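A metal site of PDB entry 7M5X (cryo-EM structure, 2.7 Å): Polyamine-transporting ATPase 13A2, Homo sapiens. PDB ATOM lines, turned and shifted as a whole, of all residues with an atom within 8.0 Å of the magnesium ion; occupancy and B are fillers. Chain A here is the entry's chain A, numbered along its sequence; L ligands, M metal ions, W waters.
Merely in contact with the magnesium ion: Gly 879 (3.9 Å). Four residues have an atom within 4 Å of the magnesium ion: Asp 513, Thr 515, Asp 878 and Gly 879.
OD1 of Asp 513 binds BE1 of the ligand (2.0 Å). F1 of the ligand is in hydrogen-bond range of OG1 of Thr 750, at 2.5 Å. N of Thr 515 lies close to F2 of the ligand, 3.3 Å away. F3 of the ligand lies within hydrogen-bond range of N of Gly 751, 3.2 Å away. A fluorine (F3) of the ligand sits at hydrogen-bond distance from the side-chain amino group of Lys 859 (3.2 Å). F3 of the ligand is in hydrogen-bond range of ND2 of Asn 881, 2.8 Å away.
Water W1 lies within hydrogen-bond range of OD1 of Asn 881, N of Gly 879 and OD2 of Asp 882.
The magnesium ion is bound by OD2 of Asp 513, O of Thr 515 and OD1 of Asp 878. The magnesium ion has three donor atoms within binding distance. Slightly farther from the magnesium ion lies water W1 (2.8 Å).
The side-chain carboxylate (OD1) of Asp 513 sits close to the side-chain amino group (NZ) of Lys 859, 3.0 Å away. The side-chain carboxylate (OD2) of Asp 882 sits at hydrogen-bond distance from the backbone NH (N) of Asp 878 (3.4 Å). OD1 of Asp 878 sits close to OG1 of Thr 517 (3.3 Å). OG1 of Thr 515 lies within hydrogen-bond range of NZ of Lys 514, 3.5 Å away. The side-chain carboxylate (OD1) of Asp 882 lies within hydrogen-bond range of the backbone NH (N) of Gly 879 (3.1 Å).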
ATOM      1  N   SER A 343      -9.202   4.256  30.982  1.00  0.00           N
ATOM      2  CA  SER A 343      -9.735   4.401  29.636  1.00  0.00           C
ATOM      3  C   SER A 343      -8.657   4.826  28.643  1.00  0.00           C
ATOM      4  O   SER A 343      -8.848   4.692  27.442  1.00  0.00           O
ATOM      5  CB  SER A 343     -10.864   5.423  29.622  1.00  0.00           C
ATOM      6  OG  SER A 343     -10.381   6.719  29.898  1.00  0.00           O
ATOM      7  N   THR A 346      -6.886   0.878  27.977  1.00  0.00           N
ATOM      8  CA  THR A 346      -7.770  -0.185  27.519  1.00  0.00           C
ATOM      9  C   THR A 346      -8.955   0.326  26.712  1.00  0.00           C
ATOM     10  O   THR A 346      -9.524  -0.449  25.944  1.00  0.00           O
ATOM     11  CB  THR A 346      -8.285  -0.983  28.718  1.00  0.00           C
ATOM     12  OG1 THR A 346      -9.297  -0.229  29.396  1.00  0.00           O
ATOM     13  CG2 THR A 346      -7.155  -1.300  29.681  1.00  0.00           C
ATOM     14  N   GLY A 347      -9.330   1.594  26.869  1.00  0.00           N
ATOM     15  CA  GLY A 347     -10.488   2.133  26.196  1.00  0.00           C
ATOM     16  C   GLY A 347     -11.796   1.994  26.965  1.00  0.00           C
ATOM     17  O   GLY A 347     -12.816   2.513  26.498  1.00  0.00           O
ATOM     18  N   GLU A 348     -11.783   1.331  28.119  1.00  0.00           N
ATOM     19  CA  GLU A 348     -12.966   1.182  28.951  1.00  0.00           C
ATOM     20  C   GLU A 348     -12.862   2.077  30.175  1.00  0.00           C
ATOM     21  O   GLU A 348     -11.767   2.286  30.714  1.00  0.00           O
ATOM     22  CB  GLU A 348     -13.148  -0.278  29.391  1.00  0.00           C
ATOM     23  CG  GLU A 348     -13.471  -1.210  28.238  1.00  0.00           C
ATOM     24  CD  GLU A 348     -12.244  -1.654  27.483  1.00  0.00           C
ATOM     25  OE1 GLU A 348     -11.125  -1.284  27.889  1.00  0.00           O
ATOM     26  OE2 GLU A 348     -12.389  -2.351  26.459  1.00  0.00           O
ATOM     27  N   PHE A 512     -11.387  -1.293  13.503  1.00  0.00           N
ATOM     28  CA  PHE A 512     -12.370  -0.556  14.284  1.00  0.00           C
ATOM     29  C   PHE A 512     -12.160  -0.835  15.759  1.00  0.00           C
ATOM     30  O   PHE A 512     -12.101  -2.001  16.173  1.00  0.00           O
ATOM     31  CB  PHE A 512     -13.785  -0.934  13.886  1.00  0.00           C
ATOM     32  CG  PHE A 512     -14.141  -0.561  12.470  1.00  0.00           C
ATOM     33  CD1 PHE A 512     -14.494   0.733  12.160  1.00  0.00           C
ATOM     34  CD2 PHE A 512     -14.135  -1.515  11.471  1.00  0.00           C
ATOM     35  CE1 PHE A 512     -14.821   1.074  10.863  1.00  0.00           C
ATOM     36  CE2 PHE A 512     -14.464  -1.177  10.184  1.00  0.00           C
ATOM     37  CZ  PHE A 512     -14.806   0.119   9.875  1.00  0.00           C
ATOM     38  N   ASP A 513     -12.050   0.221  16.547  1.00  0.00           N
ATOM     39  CA  ASP A 513     -12.148   0.098  17.986  1.00  0.00           C
ATOM     40  C   ASP A 513     -13.571  -0.298  18.360  1.00  0.00           C
ATOM     41  O   ASP A 513     -14.521  -0.028  17.622  1.00  0.00           O
ATOM     42  CB  ASP A 513     -11.755   1.414  18.651  1.00  0.00           C
ATOM     43  CG  ASP A 513     -11.736   1.331  20.154  1.00  0.00           C
ATOM     44  OD1 ASP A 513     -10.964   0.516  20.698  1.00  0.00           O
ATOM     45  OD2 ASP A 513     -12.488   2.092  20.799  1.00  0.00           O
ATOM     46  N   LYS A 514     -13.719  -0.968  19.495  1.00  0.00           N
ATOM     47  CA  LYS A 514     -15.041  -1.445  19.900  1.00  0.00           C
ATOM     48  C   LYS A 514     -15.783  -0.398  20.720  1.00  0.00           C
ATOM     49  O   LYS A 514     -16.831   0.101  20.318  1.00  0.00           O
ATOM     50  CB  LYS A 514     -14.909  -2.752  20.680  1.00  0.00           C
ATOM     51  CG  LYS A 514     -16.231  -3.474  20.871  1.00  0.00           C
ATOM     52  CD  LYS A 514     -16.050  -4.794  21.612  1.00  0.00           C
ATOM     53  CE  LYS A 514     -15.662  -4.597  23.078  1.00  0.00           C
ATOM     54  NZ  LYS A 514     -16.566  -3.679  23.818  1.00  0.00           N
ATOM     55  N   THR A 515     -15.232  -0.048  21.878  1.00  0.00           N
ATOM     56  CA  THR A 515     -15.934   0.863  22.783  1.00  0.00           C
ATOM     57  C   THR A 515     -15.881   2.282  22.226  1.00  0.00           C
ATOM     58  O   THR A 515     -14.800   2.789  21.895  1.00  0.00           O
ATOM     59  CB  THR A 515     -15.311   0.820  24.174  1.00  0.00           C
ATOM     60  OG1 THR A 515     -15.302  -0.527  24.652  1.00  0.00           O
ATOM     61  CG2 THR A 515     -16.107   1.688  25.141  1.00  0.00           C
ATOM     62  N   GLY A 516     -17.036   2.910  22.133  1.00  0.00           N
ATOM     63  CA  GLY A 516     -17.116   4.289  21.687  1.00  0.00           C
ATOM     64  C   GLY A 516     -17.227   4.438  20.179  1.00  0.00           C
ATOM     65  O   GLY A 516     -17.894   5.362  19.704  1.00  0.00           O
ATOM     66  N   THR A 517     -16.602   3.538  19.435  1.00  0.00           N
ATOM     67  CA  THR A 517     -16.620   3.580  17.974  1.00  0.00           C
ATOM     68  C   THR A 517     -17.748   2.723  17.406  1.00  0.00           C
ATOM     69  O   THR A 517     -18.632   3.236  16.714  1.00  0.00           O
ATOM     70  CB  THR A 517     -15.267   3.125  17.426  1.00  0.00           C
ATOM     71  OG1 THR A 517     -14.265   4.098  17.739  1.00  0.00           O
ATOM     72  CG2 THR A 517     -15.319   2.910  15.918  1.00  0.00           C
ATOM     73  N   LEU A 518     -17.728   1.424  17.680  1.00  0.00           N
ATOM     74  CA  LEU A 518     -18.771   0.531  17.206  1.00  0.00           C
ATOM     75  C   LEU A 518     -19.943   0.449  18.169  1.00  0.00           C
ATOM     76  O   LEU A 518     -21.066   0.189  17.738  1.00  0.00           O
ATOM     77  CB  LEU A 518     -18.201  -0.872  16.984  1.00  0.00           C
ATOM     78  CG  LEU A 518     -17.146  -1.012  15.882  1.00  0.00           C
ATOM     79  CD1 LEU A 518     -16.418  -2.331  16.029  1.00  0.00           C
ATOM     80  CD2 LEU A 518     -17.793  -0.906  14.514  1.00  0.00           C
ATOM     81  N   THR A 519     -19.693   0.646  19.465  1.00  0.00           N
ATOM     82  CA  THR A 519     -20.714   0.578  20.500  1.00  0.00           C
ATOM     83  C   THR A 519     -20.744   1.895  21.254  1.00  0.00           C
ATOM     84  O   THR A 519     -19.810   2.704  21.169  1.00  0.00           O
ATOM     85  CB  THR A 519     -20.438  -0.586  21.465  1.00  0.00           C
ATOM     86  OG1 THR A 519     -19.218  -0.345  22.161  1.00  0.00           O
ATOM     87  CG2 THR A 519     -20.337  -1.899  20.709  1.00  0.00           C
ATOM     88  N   GLU A 520     -21.819   2.099  22.008  1.00  0.00           N
ATOM     89  CA  GLU A 520     -21.930   3.320  22.793  1.00  0.00           C
ATOM     90  C   GLU A 520     -20.812   3.382  23.827  1.00  0.00           C
ATOM     91  O   GLU A 520     -20.335   2.353  24.318  1.00  0.00           O
ATOM     92  CB  GLU A 520     -23.292   3.385  23.493  1.00  0.00           C
ATOM     93  CG  GLU A 520     -24.366   4.131  22.713  1.00  0.00           C
ATOM     94  CD  GLU A 520     -24.980   3.295  21.615  1.00  0.00           C
ATOM     95  OE1 GLU A 520     -24.998   2.052  21.743  1.00  0.00           O
ATOM     96  OE2 GLU A 520     -25.451   3.877  20.611  1.00  0.00           O
ATOM     97  N   ASP A 521     -20.395   4.600  24.159  1.00  0.00           N
ATOM     98  CA  ASP A 521     -19.320   4.806  25.120  1.00  0.00           C
ATOM     99  C   ASP A 521     -19.859   4.705  26.539  1.00  0.00           C
ATOM    100  O   ASP A 521     -19.865   5.665  27.322  1.00  0.00           O
ATOM    101  CB  ASP A 521     -18.644   6.156  24.860  1.00  0.00           C
ATOM    102  CG  ASP A 521     -17.381   6.336  25.680  1.00  0.00           C
ATOM    103  OD1 ASP A 521     -17.040   5.434  26.467  1.00  0.00           O
ATOM    104  OD2 ASP A 521     -16.722   7.389  25.521  1.00  0.00           O
ATOM    105  N   LYS A 729     -23.971   0.850  18.235  1.00  0.00           N
ATOM    106  CA  LYS A 729     -24.533   2.112  17.791  1.00  0.00           C
ATOM    107  C   LYS A 729     -25.544   1.839  16.676  1.00  0.00           C
ATOM    108  O   LYS A 729     -25.407   0.852  15.941  1.00  0.00           O
ATOM    109  CB  LYS A 729     -23.452   3.060  17.310  1.00  0.00           C
ATOM    110  CG  LYS A 729     -22.920   3.965  18.396  1.00  0.00           C
ATOM    111  CD  LYS A 729     -21.604   4.594  18.006  1.00  0.00           C
ATOM    112  CE  LYS A 729     -21.141   5.578  19.051  1.00  0.00           C
ATOM    113  NZ  LYS A 729     -19.769   6.078  18.771  1.00  0.00           N
ATOM    114  N   VAL A 749     -10.239  -4.248  16.751  1.00  0.00           N
ATOM    115  CA  VAL A 749      -9.049  -4.113  17.572  1.00  0.00           C
ATOM    116  C   VAL A 749      -9.446  -3.285  18.788  1.00  0.00           C
ATOM    117  O   VAL A 749      -9.600  -2.072  18.687  1.00  0.00           O
ATOM    118  CB  VAL A 749      -7.892  -3.444  16.813  1.00  0.00           C
ATOM    119  CG1 VAL A 749      -6.585  -3.609  17.583  1.00  0.00           C
ATOM    120  CG2 VAL A 749      -7.765  -4.035  15.419  1.00  0.00           C
ATOM    121  N   THR A 750      -9.621  -3.969  19.917  1.00  0.00           N
ATOM    122  CA  THR A 750     -10.312  -3.563  21.175  1.00  0.00           C
ATOM    123  C   THR A 750      -9.276  -3.756  22.293  1.00  0.00           C
ATOM    124  O   THR A 750      -8.490  -4.620  22.092  1.00  0.00           O
ATOM    125  CB  THR A 750     -11.634  -4.326  21.272  1.00  0.00           C
ATOM    126  OG1 THR A 750     -12.378  -4.015  22.440  1.00  0.00           O
ATOM    127  CG2 THR A 750     -11.545  -5.830  21.306  1.00  0.00           C
ATOM    128  N   GLY A 751      -9.294  -3.005  23.396  1.00  0.00           N
ATOM    129  CA  GLY A 751      -8.712  -3.372  24.661  1.00  0.00           C
ATOM    130  C   GLY A 751      -9.625  -4.126  25.591  1.00  0.00           C
ATOM    131  O   GLY A 751      -9.232  -4.407  26.723  1.00  0.00           O
ATOM    132  N   LYS A 859      -1.779  -2.253  19.117  1.00  0.00           N
ATOM    133  CA  LYS A 859      -2.565  -1.805  17.964  1.00  0.00           C
ATOM    134  C   LYS A 859      -1.652  -1.274  16.866  1.00  0.00           C
ATOM    135  O   LYS A 859      -1.817  -1.597  15.693  1.00  0.00           O
ATOM    136  CB  LYS A 859      -3.562  -0.745  18.408  1.00  0.00           C
ATOM    137  CG  LYS A 859      -4.473  -1.188  19.538  1.00  0.00           C
ATOM    138  CD  LYS A 859      -5.756  -0.382  19.559  1.00  0.00           C
ATOM    139  CE  LYS A 859      -6.696  -0.863  20.646  1.00  0.00           C
ATOM    140  NZ  LYS A 859      -7.990  -0.133  20.626  1.00  0.00           N
ATOM    141  N   MET A 875      -7.998   3.036  10.027  1.00  0.00           N
ATOM    142  CA  MET A 875      -8.593   2.713  11.313  1.00  0.00           C
ATOM    143  C   MET A 875      -9.483   3.867  11.761  1.00  0.00           C
ATOM    144  O   MET A 875      -9.202   5.032  11.465  1.00  0.00           O
ATOM    145  CB  MET A 875      -7.521   2.417  12.368  1.00  0.00           C
ATOM    146  CG  MET A 875      -8.056   2.297  13.783  1.00  0.00           C
ATOM    147  SD  MET A 875      -7.124   1.113  14.761  1.00  0.00           S
ATOM    148  CE  MET A 875      -7.759   1.479  16.388  1.00  0.00           C
ATOM    149  N   CYS A 876     -10.555   3.527  12.475  1.00  0.00           N
ATOM    150  CA  CYS A 876     -11.550   4.475  12.954  1.00  0.00           C
ATOM    151  C   CYS A 876     -11.613   4.507  14.477  1.00  0.00           C
ATOM    152  O   CYS A 876     -12.695   4.516  15.068  1.00  0.00           O
ATOM    153  CB  CYS A 876     -12.926   4.146  12.376  1.00  0.00           C
ATOM    154  SG  CYS A 876     -14.106   5.497  12.479  1.00  0.00           S
ATOM    155  N   GLY A 877     -10.465   4.535  15.133  1.00  0.00           N
ATOM    156  CA  GLY A 877     -10.447   4.630  16.586  1.00  0.00           C
ATOM    157  C   GLY A 877     -11.022   5.939  17.084  1.00  0.00           C
ATOM    158  O   GLY A 877     -11.165   6.914  16.335  1.00  0.00           O
ATOM    159  N   ASP A 878     -11.347   5.962  18.370  1.00  0.00           N
ATOM    160  CA  ASP A 878     -11.930   7.148  18.992  1.00  0.00           C
ATOM    161  C   ASP A 878     -11.231   7.537  20.290  1.00  0.00           C
ATOM    162  O   ASP A 878     -11.180   8.722  20.638  1.00  0.00           O
ATOM    163  CB  ASP A 878     -13.419   6.926  19.277  1.00  0.00           C
ATOM    164  CG  ASP A 878     -13.662   6.036  20.472  1.00  0.00           C
ATOM    165  OD1 ASP A 878     -12.961   5.005  20.614  1.00  0.00           O
ATOM    166  OD2 ASP A 878     -14.535   6.379  21.292  1.00  0.00           O
ATOM    167  N   GLY A 879     -10.683   6.556  21.008  1.00  0.00           N
ATOM    168  CA  GLY A 879     -10.136   6.784  22.333  1.00  0.00           C
ATOM    169  C   GLY A 879      -8.687   7.225  22.294  1.00  0.00           C
ATOM    170  O   GLY A 879      -8.070   7.395  21.241  1.00  0.00           O
ATOM    171  N   ALA A 880      -8.136   7.421  23.487  1.00  0.00           N
ATOM    172  CA  ALA A 880      -6.732   7.792  23.623  1.00  0.00           C
ATOM    173  C   ALA A 880      -5.808   6.606  23.399  1.00  0.00           C
ATOM    174  O   ALA A 880      -4.684   6.786  22.930  1.00  0.00           O
ATOM    175  CB  ALA A 880      -6.479   8.390  24.997  1.00  0.00           C
ATOM    176  N   ASN A 881      -6.260   5.389  23.725  1.00  0.00           N
ATOM    177  CA  ASN A 881      -5.413   4.219  23.590  1.00  0.00           C
ATOM    178  C   ASN A 881      -5.037   3.986  22.124  1.00  0.00           C
ATOM    179  O   ASN A 881      -3.882   3.645  21.821  1.00  0.00           O
ATOM    180  CB  ASN A 881      -6.102   2.984  24.167  1.00  0.00           C
ATOM    181  CG  ASN A 881      -7.490   2.775  23.596  1.00  0.00           C
ATOM    182  OD1 ASN A 881      -8.230   3.732  23.380  1.00  0.00           O
ATOM    183  ND2 ASN A 881      -7.864   1.522  23.363  1.00  0.00           N
ATOM    184  N   ASP A 882      -5.988   4.158  21.217  1.00  0.00           N
ATOM    185  CA  ASP A 882      -5.751   3.918  19.796  1.00  0.00           C
ATOM    186  C   ASP A 882      -5.415   5.237  19.099  1.00  0.00           C
ATOM    187  O   ASP A 882      -6.168   5.753  18.276  1.00  0.00           O
ATOM    188  CB  ASP A 882      -6.949   3.240  19.161  1.00  0.00           C
ATOM    189  CG  ASP A 882      -8.254   3.954  19.437  1.00  0.00           C
ATOM    190  OD1 ASP A 882      -8.219   5.086  19.956  1.00  0.00           O
ATOM    191  OD2 ASP A 882      -9.324   3.381  19.141  1.00  0.00           O
ATOM    192  N   LEU A 895     -13.187   9.781  15.872  1.00  0.00           N
ATOM    193  CA  LEU A 895     -14.552  10.140  16.188  1.00  0.00           C
ATOM    194  C   LEU A 895     -14.656  11.069  17.399  1.00  0.00           C
ATOM    195  O   LEU A 895     -15.750  11.549  17.690  1.00  0.00           O
ATOM    196  CB  LEU A 895     -15.384   8.875  16.442  1.00  0.00           C
ATOM    197  CG  LEU A 895     -15.305   7.810  15.351  1.00  0.00           C
ATOM    198  CD1 LEU A 895     -16.169   6.626  15.725  1.00  0.00           C
ATOM    199  CD2 LEU A 895     -15.735   8.381  14.007  1.00  0.00           C
HETATM  200 BE1  LIG L   1     -11.703  -0.074  22.494  1.00  0.00          BE
HETATM  201  F1  LIG L   1     -12.237  -1.494  22.772  1.00  0.00           F
HETATM  202  F2  LIG L   1     -12.472   1.025  23.292  1.00  0.00           F
HETATM  203  F3  LIG L   1     -10.218   0.003  22.897  1.00  0.00           F
HETATM  204 MG    MG M   1     -12.987   3.562  21.997  1.00  0.00          MG
HETATM  205  O   HOH W   1     -10.250   3.940  21.975  1.00  0.00           O
